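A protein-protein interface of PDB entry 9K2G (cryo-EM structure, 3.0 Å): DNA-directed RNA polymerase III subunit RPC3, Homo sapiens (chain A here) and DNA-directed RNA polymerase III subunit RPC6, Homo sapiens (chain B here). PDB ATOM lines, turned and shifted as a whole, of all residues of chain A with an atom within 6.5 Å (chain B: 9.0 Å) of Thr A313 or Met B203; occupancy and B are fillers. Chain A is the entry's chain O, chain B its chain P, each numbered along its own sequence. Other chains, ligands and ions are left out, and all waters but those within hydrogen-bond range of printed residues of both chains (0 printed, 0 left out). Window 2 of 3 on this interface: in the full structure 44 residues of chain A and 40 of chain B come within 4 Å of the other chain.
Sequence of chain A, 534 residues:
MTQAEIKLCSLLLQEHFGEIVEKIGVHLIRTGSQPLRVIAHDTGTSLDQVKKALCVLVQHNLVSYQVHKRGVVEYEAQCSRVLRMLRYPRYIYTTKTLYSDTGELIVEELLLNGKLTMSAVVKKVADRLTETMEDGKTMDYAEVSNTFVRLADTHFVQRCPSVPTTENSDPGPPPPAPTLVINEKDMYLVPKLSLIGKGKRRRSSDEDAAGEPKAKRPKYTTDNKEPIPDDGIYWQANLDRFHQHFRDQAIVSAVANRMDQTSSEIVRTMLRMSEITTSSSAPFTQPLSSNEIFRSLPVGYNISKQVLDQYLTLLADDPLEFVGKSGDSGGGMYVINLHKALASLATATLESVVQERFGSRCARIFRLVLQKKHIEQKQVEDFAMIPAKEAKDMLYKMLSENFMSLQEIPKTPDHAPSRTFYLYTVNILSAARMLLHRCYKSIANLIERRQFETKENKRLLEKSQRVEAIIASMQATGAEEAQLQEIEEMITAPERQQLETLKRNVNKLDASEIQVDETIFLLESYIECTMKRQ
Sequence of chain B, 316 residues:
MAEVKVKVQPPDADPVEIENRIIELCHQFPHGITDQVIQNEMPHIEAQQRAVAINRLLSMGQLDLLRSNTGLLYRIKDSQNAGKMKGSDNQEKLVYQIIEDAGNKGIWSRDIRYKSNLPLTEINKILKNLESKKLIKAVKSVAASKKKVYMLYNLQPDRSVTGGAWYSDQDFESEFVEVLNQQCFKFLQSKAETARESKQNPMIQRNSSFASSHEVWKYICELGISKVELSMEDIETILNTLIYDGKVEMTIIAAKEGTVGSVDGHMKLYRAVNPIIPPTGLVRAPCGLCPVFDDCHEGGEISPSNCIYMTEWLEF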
ATOM      1  N   LEU A 308      22.004  16.503 -15.212  1.00  0.00           N
ATOM      2  CA  LEU A 308      21.248  17.022 -14.074  1.00  0.00           C
ATOM      3  C   LEU A 308      21.608  18.472 -13.785  1.00  0.00           C
ATOM      4  O   LEU A 308      20.729  19.286 -13.487  1.00  0.00           O
ATOM      5  CB  LEU A 308      21.497  16.159 -12.838  1.00  0.00           C
ATOM      6  CG  LEU A 308      20.938  16.745 -11.538  1.00  0.00           C
ATOM      7  CD1 LEU A 308      19.421  16.866 -11.582  1.00  0.00           C
ATOM      8  CD2 LEU A 308      21.374  15.925 -10.343  1.00  0.00           C
ATOM      9  N   ASP A 309      22.895  18.811 -13.862  1.00  0.00           N
ATOM     10  CA  ASP A 309      23.297  20.198 -13.635  1.00  0.00           C
ATOM     11  C   ASP A 309      22.730  21.120 -14.707  1.00  0.00           C
ATOM     12  O   ASP A 309      22.307  22.244 -14.408  1.00  0.00           O
ATOM     13  CB  ASP A 309      24.822  20.302 -13.578  1.00  0.00           C
ATOM     14  CG  ASP A 309      25.303  21.695 -13.233  1.00  0.00           C
ATOM     15  OD1 ASP A 309      25.293  22.572 -14.124  1.00  0.00           O
ATOM     16  OD2 ASP A 309      25.681  21.925 -12.063  1.00  0.00           O
ATOM     17  N   GLN A 310      22.714  20.659 -15.962  1.00  0.00           N
ATOM     18  CA  GLN A 310      22.104  21.436 -17.036  1.00  0.00           C
ATOM     19  C   GLN A 310      20.624  21.666 -16.766  1.00  0.00           C
ATOM     20  O   GLN A 310      20.118  22.785 -16.925  1.00  0.00           O
ATOM     21  CB  GLN A 310      22.296  20.723 -18.377  1.00  0.00           C
ATOM     22  CG  GLN A 310      23.698  20.814 -18.954  1.00  0.00           C
ATOM     23  CD  GLN A 310      23.794  20.183 -20.331  1.00  0.00           C
ATOM     24  OE1 GLN A 310      22.803  19.695 -20.873  1.00  0.00           O
ATOM     25  NE2 GLN A 310      24.989  20.194 -20.904  1.00  0.00           N
ATOM     26  N   TYR A 311      19.913  20.614 -16.347  1.00  0.00           N
ATOM     27  CA  TYR A 311      18.495  20.756 -16.028  1.00  0.00           C
ATOM     28  C   TYR A 311      18.294  21.757 -14.900  1.00  0.00           C
ATOM     29  O   TYR A 311      17.419  22.626 -14.971  1.00  0.00           O
ATOM     30  CB  TYR A 311      17.901  19.401 -15.651  1.00  0.00           C
ATOM     31  CG  TYR A 311      17.546  18.526 -16.829  1.00  0.00           C
ATOM     32  CD1 TYR A 311      17.346  19.076 -18.088  1.00  0.00           C
ATOM     33  CD2 TYR A 311      17.402  17.152 -16.684  1.00  0.00           C
ATOM     34  CE1 TYR A 311      17.016  18.282 -19.166  1.00  0.00           C
ATOM     35  CE2 TYR A 311      17.073  16.348 -17.755  1.00  0.00           C
ATOM     36  CZ  TYR A 311      16.883  16.919 -19.000  1.00  0.00           C
ATOM     37  OH  TYR A 311      16.556  16.122 -20.073  1.00  0.00           O
ATOM     38  N   LEU A 312      19.107  21.649 -13.846  1.00  0.00           N
ATOM     39  CA  LEU A 312      18.965  22.545 -12.703  1.00  0.00           C
ATOM     40  C   LEU A 312      19.210  23.994 -13.099  1.00  0.00           C
ATOM     41  O   LEU A 312      18.452  24.888 -12.703  1.00  0.00           O
ATOM     42  CB  LEU A 312      19.918  22.116 -11.590  1.00  0.00           C
ATOM     43  CG  LEU A 312      19.491  20.924 -10.732  1.00  0.00           C
ATOM     44  CD1 LEU A 312      20.671  20.380  -9.944  1.00  0.00           C
ATOM     45  CD2 LEU A 312      18.364  21.324  -9.793  1.00  0.00           C
ATOM     46  N   THR A 313      20.255  24.253 -13.889  1.00  0.00           N
ATOM     47  CA  THR A 313      20.567  25.636 -14.235  1.00  0.00           C
ATOM     48  C   THR A 313      19.600  26.197 -15.270  1.00  0.00           C
ATOM     49  O   THR A 313      19.369  27.414 -15.293  1.00  0.00           O
ATOM     50  CB  THR A 313      22.015  25.757 -14.724  1.00  0.00           C
ATOM     51  OG1 THR A 313      22.332  27.137 -14.945  1.00  0.00           O
ATOM     52  CG2 THR A 313      22.224  24.989 -16.014  1.00  0.00           C
ATOM     53  N   LEU A 314      19.024  25.354 -16.135  1.00  0.00           N
ATOM     54  CA  LEU A 314      18.044  25.866 -17.086  1.00  0.00           C
ATOM     55  C   LEU A 314      16.699  26.111 -16.420  1.00  0.00           C
ATOM     56  O   LEU A 314      15.984  27.049 -16.790  1.00  0.00           O
ATOM     57  CB  LEU A 314      17.914  24.919 -18.285  1.00  0.00           C
ATOM     58  CG  LEU A 314      17.260  23.536 -18.196  1.00  0.00           C
ATOM     59  CD1 LEU A 314      15.760  23.616 -18.423  1.00  0.00           C
ATOM     60  CD2 LEU A 314      17.895  22.592 -19.206  1.00  0.00           C
ATOM     61  N   LEU A 315      16.333  25.282 -15.437  1.00  0.00           N
ATOM     62  CA  LEU A 315      15.148  25.577 -14.637  1.00  0.00           C
ATOM     63  C   LEU A 315      15.352  26.815 -13.775  1.00  0.00           C
ATOM     64  O   LEU A 315      14.406  27.575 -13.545  1.00  0.00           O
ATOM     65  CB  LEU A 315      14.781  24.377 -13.761  1.00  0.00           C
ATOM     66  CG  LEU A 315      13.726  23.393 -14.273  1.00  0.00           C
ATOM     67  CD1 LEU A 315      14.300  22.489 -15.342  1.00  0.00           C
ATOM     68  CD2 LEU A 315      13.165  22.576 -13.122  1.00  0.00           C
ATOM     69  N   ALA A 316      16.579  27.033 -13.289  1.00  0.00           N
ATOM     70  CA  ALA A 316      16.862  28.215 -12.481  1.00  0.00           C
ATOM     71  C   ALA A 316      16.702  29.499 -13.280  1.00  0.00           C
ATOM     72  O   ALA A 316      16.414  30.558 -12.711  1.00  0.00           O
ATOM     73  CB  ALA A 316      18.269  28.129 -11.892  1.00  0.00           C
ATOM     74  N   ASP A 317      16.887  29.436 -14.597  1.00  0.00           N
ATOM     75  CA  ASP A 317      16.723  30.595 -15.467  1.00  0.00           C
ATOM     76  C   ASP A 317      15.315  30.716 -16.037  1.00  0.00           C
ATOM     77  O   ASP A 317      15.052  31.647 -16.800  1.00  0.00           O
ATOM     78  CB  ASP A 317      17.738  30.552 -16.607  1.00  0.00           C
ATOM     79  CG  ASP A 317      19.172  30.540 -16.113  1.00  0.00           C
ATOM     80  OD1 ASP A 317      19.397  30.902 -14.937  1.00  0.00           O
ATOM     81  OD2 ASP A 317      20.073  30.176 -16.897  1.00  0.00           O
ATOM     82  N   ASP A 318      14.421  29.796 -15.699  1.00  0.00           N
ATOM     83  CA  ASP A 318      13.050  29.875 -16.179  1.00  0.00           C
ATOM     84  C   ASP A 318      12.375  31.114 -15.597  1.00  0.00           C
ATOM     85  O   ASP A 318      12.423  31.324 -14.380  1.00  0.00           O
ATOM     86  CB  ASP A 318      12.279  28.613 -15.781  1.00  0.00           C
ATOM     87  CG  ASP A 318      10.985  28.442 -16.552  1.00  0.00           C
ATOM     88  OD1 ASP A 318      10.880  28.957 -17.687  1.00  0.00           O
ATOM     89  OD2 ASP A 318      10.065  27.786 -16.022  1.00  0.00           O
ATOM     90  N   TYR A 334      20.653  23.931  -4.868  1.00  0.00           N
ATOM     91  CA  TYR A 334      19.401  24.425  -5.417  1.00  0.00           C
ATOM     92  C   TYR A 334      18.281  24.331  -4.392  1.00  0.00           C
ATOM     93  O   TYR A 334      18.309  23.507  -3.479  1.00  0.00           O
ATOM     94  CB  TYR A 334      19.014  23.656  -6.686  1.00  0.00           C
ATOM     95  CG  TYR A 334      19.805  24.088  -7.898  1.00  0.00           C
ATOM     96  CD1 TYR A 334      19.333  25.078  -8.749  1.00  0.00           C
ATOM     97  CD2 TYR A 334      21.043  23.516  -8.186  1.00  0.00           C
ATOM     98  CE1 TYR A 334      20.055  25.479  -9.852  1.00  0.00           C
ATOM     99  CE2 TYR A 334      21.774  23.915  -9.284  1.00  0.00           C
ATOM    100  CZ  TYR A 334      21.274  24.895 -10.119  1.00  0.00           C
ATOM    101  OH  TYR A 334      22.001  25.293 -11.220  1.00  0.00           O
ATOM    102  N   ALA B 195      12.971  20.850 -32.747  1.00  0.00           N
ATOM    103  CA  ALA B 195      13.950  20.868 -31.666  1.00  0.00           C
ATOM    104  C   ALA B 195      13.722  19.723 -30.688  1.00  0.00           C
ATOM    105  O   ALA B 195      14.679  19.080 -30.243  1.00  0.00           O
ATOM    106  CB  ALA B 195      13.898  22.214 -30.941  1.00  0.00           C
ATOM    107  N   SER B 198      14.787  16.493 -32.260  1.00  0.00           N
ATOM    108  CA  SER B 198      16.237  16.392 -32.399  1.00  0.00           C
ATOM    109  C   SER B 198      16.860  15.675 -31.212  1.00  0.00           C
ATOM    110  O   SER B 198      17.786  14.873 -31.377  1.00  0.00           O
ATOM    111  CB  SER B 198      16.846  17.783 -32.566  1.00  0.00           C
ATOM    112  OG  SER B 198      16.641  18.577 -31.413  1.00  0.00           O
ATOM    113  N   LYS B 199      16.378  15.973 -29.999  1.00  0.00           N
ATOM    114  CA  LYS B 199      16.806  15.369 -28.735  1.00  0.00           C
ATOM    115  C   LYS B 199      18.321  15.224 -28.631  1.00  0.00           C
ATOM    116  O   LYS B 199      18.820  14.283 -28.002  1.00  0.00           O
ATOM    117  CB  LYS B 199      16.116  14.010 -28.515  1.00  0.00           C
ATOM    118  CG  LYS B 199      16.474  12.899 -29.498  1.00  0.00           C
ATOM    119  CD  LYS B 199      15.646  11.652 -29.262  1.00  0.00           C
ATOM    120  CE  LYS B 199      15.967  10.573 -30.283  1.00  0.00           C
ATOM    121  NZ  LYS B 199      17.414  10.218 -30.263  1.00  0.00           N
ATOM    122  N   GLN B 200      19.062  16.162 -29.223  1.00  0.00           N
ATOM    123  CA  GLN B 200      20.521  16.091 -29.194  1.00  0.00           C
ATOM    124  C   GLN B 200      21.063  16.423 -27.810  1.00  0.00           C
ATOM    125  O   GLN B 200      21.914  15.703 -27.277  1.00  0.00           O
ATOM    126  CB  GLN B 200      21.104  17.026 -30.253  1.00  0.00           C
ATOM    127  CG  GLN B 200      22.613  16.947 -30.406  1.00  0.00           C
ATOM    128  CD  GLN B 200      23.328  18.041 -29.646  1.00  0.00           C
ATOM    129  OE1 GLN B 200      22.701  18.846 -28.964  1.00  0.00           O
ATOM    130  NE2 GLN B 200      24.649  18.082 -29.769  1.00  0.00           N
ATOM    131  N   ASN B 201      20.570  17.509 -27.207  1.00  0.00           N
ATOM    132  CA  ASN B 201      20.959  17.936 -25.864  1.00  0.00           C
ATOM    133  C   ASN B 201      20.008  19.031 -25.394  1.00  0.00           C
ATOM    134  O   ASN B 201      19.640  19.912 -26.186  1.00  0.00           O
ATOM    135  CB  ASN B 201      22.407  18.430 -25.850  1.00  0.00           C
ATOM    136  CG  ASN B 201      22.940  18.636 -24.447  1.00  0.00           C
ATOM    137  OD1 ASN B 201      23.445  17.710 -23.816  1.00  0.00           O
ATOM    138  ND2 ASN B 201      22.825  19.865 -23.952  1.00  0.00           N
ATOM    139  N   PRO B 202      19.591  19.013 -24.120  1.00  0.00           N
ATOM    140  CA  PRO B 202      18.561  19.971 -23.675  1.00  0.00           C
ATOM    141  C   PRO B 202      18.914  21.429 -23.919  1.00  0.00           C
ATOM    142  O   PRO B 202      18.046  22.212 -24.323  1.00  0.00           O
ATOM    143  CB  PRO B 202      18.429  19.659 -22.175  1.00  0.00           C
ATOM    144  CG  PRO B 202      18.864  18.233 -22.052  1.00  0.00           C
ATOM    145  CD  PRO B 202      19.951  18.053 -23.064  1.00  0.00           C
ATOM    146  N   MET B 203      20.172  21.814 -23.703  1.00  0.00           N
ATOM    147  CA  MET B 203      20.582  23.188 -23.992  1.00  0.00           C
ATOM    148  C   MET B 203      20.437  23.497 -25.474  1.00  0.00           C
ATOM    149  O   MET B 203      19.841  24.513 -25.857  1.00  0.00           O
ATOM    150  CB  MET B 203      22.021  23.409 -23.537  1.00  0.00           C
ATOM    151  CG  MET B 203      22.211  23.322 -22.033  1.00  0.00           C
ATOM    152  SD  MET B 203      21.322  24.616 -21.151  1.00  0.00           S
ATOM    153  CE  MET B 203      21.712  24.187 -19.459  1.00  0.00           C
ATOM    154  N   ILE B 204      20.970  22.620 -26.324  1.00  0.00           N
ATOM    155  CA  ILE B 204      20.875  22.823 -27.765  1.00  0.00           C
ATOM    156  C   ILE B 204      19.429  22.709 -28.229  1.00  0.00           C
ATOM    157  O   ILE B 204      18.999  23.431 -29.134  1.00  0.00           O
ATOM    158  CB  ILE B 204      21.799  21.837 -28.505  1.00  0.00           C
ATOM    159  CG1 ILE B 204      23.272  22.175 -28.248  1.00  0.00           C
ATOM    160  CG2 ILE B 204      21.524  21.852 -29.997  1.00  0.00           C
ATOM    161  CD1 ILE B 204      23.870  21.520 -27.020  1.00  0.00           C
ATOM    162  N   GLN B 205      18.652  21.812 -27.612  1.00  0.00           N
ATOM    163  CA  GLN B 205      17.238  21.703 -27.951  1.00  0.00           C
ATOM    164  C   GLN B 205      16.510  23.018 -27.691  1.00  0.00           C
ATOM    165  O   GLN B 205      15.771  23.514 -28.547  1.00  0.00           O
ATOM    166  CB  GLN B 205      16.590  20.567 -27.160  1.00  0.00           C
ATOM    167  CG  GLN B 205      16.983  19.174 -27.617  1.00  0.00           C
ATOM    168  CD  GLN B 205      16.595  18.105 -26.613  1.00  0.00           C
ATOM    169  OE1 GLN B 205      17.433  17.318 -26.172  1.00  0.00           O
ATOM    170  NE2 GLN B 205      15.319  18.069 -26.248  1.00  0.00           N
ATOM    171  N   ARG B 206      16.719  23.602 -26.506  1.00  0.00           N
ATOM    172  CA  ARG B 206      16.067  24.867 -26.185  1.00  0.00           C
ATOM    173  C   ARG B 206      16.562  25.995 -27.088  1.00  0.00           C
ATOM    174  O   ARG B 206      15.764  26.827 -27.537  1.00  0.00           O
ATOM    175  CB  ARG B 206      16.299  25.222 -24.714  1.00  0.00           C
ATOM    176  CG  ARG B 206      15.534  24.343 -23.736  1.00  0.00           C
ATOM    177  CD  ARG B 206      14.034  24.561 -23.855  1.00  0.00           C
ATOM    178  NE  ARG B 206      13.660  25.942 -23.566  1.00  0.00           N
ATOM    179  CZ  ARG B 206      13.412  26.412 -22.350  1.00  0.00           C
ATOM    180  NH1 ARG B 206      13.493  25.636 -21.284  1.00  0.00           N
ATOM    181  NH2 ARG B 206      13.077  27.688 -22.204  1.00  0.00           N
ATOM    182  N   ASN B 207      17.865  26.039 -27.365  1.00  0.00           N
ATOM    183  CA  ASN B 207      18.403  27.106 -28.208  1.00  0.00           C
ATOM    184  C   ASN B 207      17.879  27.015 -29.632  1.00  0.00           C
ATOM    185  O   ASN B 207      17.561  28.037 -30.250  1.00  0.00           O
ATOM    186  CB  ASN B 207      19.931  27.074 -28.184  1.00  0.00           C
ATOM    187  CG  ASN B 207      20.499  27.400 -26.818  1.00  0.00           C
ATOM    188  OD1 ASN B 207      21.446  26.760 -26.359  1.00  0.00           O
ATOM    189  ND2 ASN B 207      19.915  28.392 -26.156  1.00  0.00           N
ATOM    190  N   SER B 208      17.784  25.798 -30.181  1.00  0.00           N
ATOM    191  CA  SER B 208      17.247  25.632 -31.528  1.00  0.00           C
ATOM    192  C   SER B 208      15.747  25.876 -31.564  1.00  0.00           C
ATOM    193  O   SER B 208      15.219  26.328 -32.588  1.00  0.00           O
ATOM    194  CB  SER B 208      17.573  24.235 -32.060  1.00  0.00           C
ATOM    195  OG  SER B 208      16.974  23.229 -31.260  1.00  0.00           O
ATOM    196  N   SER B 209      15.038  25.574 -30.475  1.00  0.00           N
ATOM    197  CA  SER B 209      13.624  25.926 -30.401  1.00  0.00           C
ATOM    198  C   SER B 209      13.430  27.434 -30.413  1.00  0.00           C
ATOM    199  O   SER B 209      12.412  27.924 -30.908  1.00  0.00           O
ATOM    200  CB  SER B 209      12.996  25.315 -29.148  1.00  0.00           C
ATOM    201  OG  SER B 209      13.524  25.903 -27.973  1.00  0.00           O
ATOM    202  N   PHE B 210      14.391  28.178 -29.875  1.00  0.00           N
ATOM    203  CA  PHE B 210      14.342  29.632 -29.921  1.00  0.00           C
ATOM    204  C   PHE B 210      14.437  30.127 -31.358  1.00  0.00           C
ATOM    205  O   PHE B 210      15.192  29.586 -32.170  1.00  0.00           O
ATOM    206  CB  PHE B 210      15.472  30.230 -29.086  1.00  0.00           C
ATOM    207  CG  PHE B 210      15.126  30.417 -27.640  1.00  0.00           C
ATOM    208  CD1 PHE B 210      13.923  30.998 -27.268  1.00  0.00           C
ATOM    209  CD2 PHE B 210      16.007  30.023 -26.647  1.00  0.00           C
ATOM    210  CE1 PHE B 210      13.611  31.179 -25.934  1.00  0.00           C
ATOM    211  CE2 PHE B 210      15.694  30.195 -25.315  1.00  0.00           C
ATOM    212  CZ  PHE B 210      14.497  30.773 -24.957  1.00  0.00           C
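The side-chain amide oxygen (OE1) of Gln A310 lies within hydrogen-bond range of the side-chain amide nitrogen (ND2) of Asn B201.
Among the printed residues, pairs that only touch across the chains: Gln A310 with Pro B202 (3.95 Å), Gln A310 with Met B203 (3.3 Å), Tyr A311 with Pro B202 (3.4 Å) and Thr A313 with Met B203 (3.6 Å).
Of the 14 printed residues of chain B, 3 touch a printed residue of chain A.
Hydrophobic or aromatic side chains of chain A within 4 Å of the printed part of chain B: Tyr A311.
Among the printed residues, 5 pairs touch across the chains.
The backbone NH of Thr A313 is in hydrogen-bond range of the side-chain hydroxyl of Tyr A334 (3.4 Å).
The backbone NH (N) of Met B203 lies close to the side-chain amide nitrogen (ND2) of Asn B201.
The side-chain amide oxygen of Gln B205 sits close to the backbone NH of Asn B201, at 3.3 Å.
The backbone carbonyl oxygen (O) of Met B203 lies close to the side-chain amide oxygen (OD1) of Asn B207.
Thr A313 touches just one residue of chain B: Met B203.
Of chain A, only Gln A310 (3.3 Å) and Thr A313 (3.6 Å) come within 4 Å of Met B203.
Of the printed residues of chain B, Gln A310 touches Asn B201 (3.1 Å), Pro B202 (3.95 Å) and Met B203 (3.3 Å).
Of the printed residues of chain A, Asn B201 touches Gln A310.
Printed residues of chain A within 4 Å of Pro B202: Gln A310 and Tyr A311.
Printed residues of chain B within 4 Å of Tyr A311: Pro B202 (3.4 Å).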
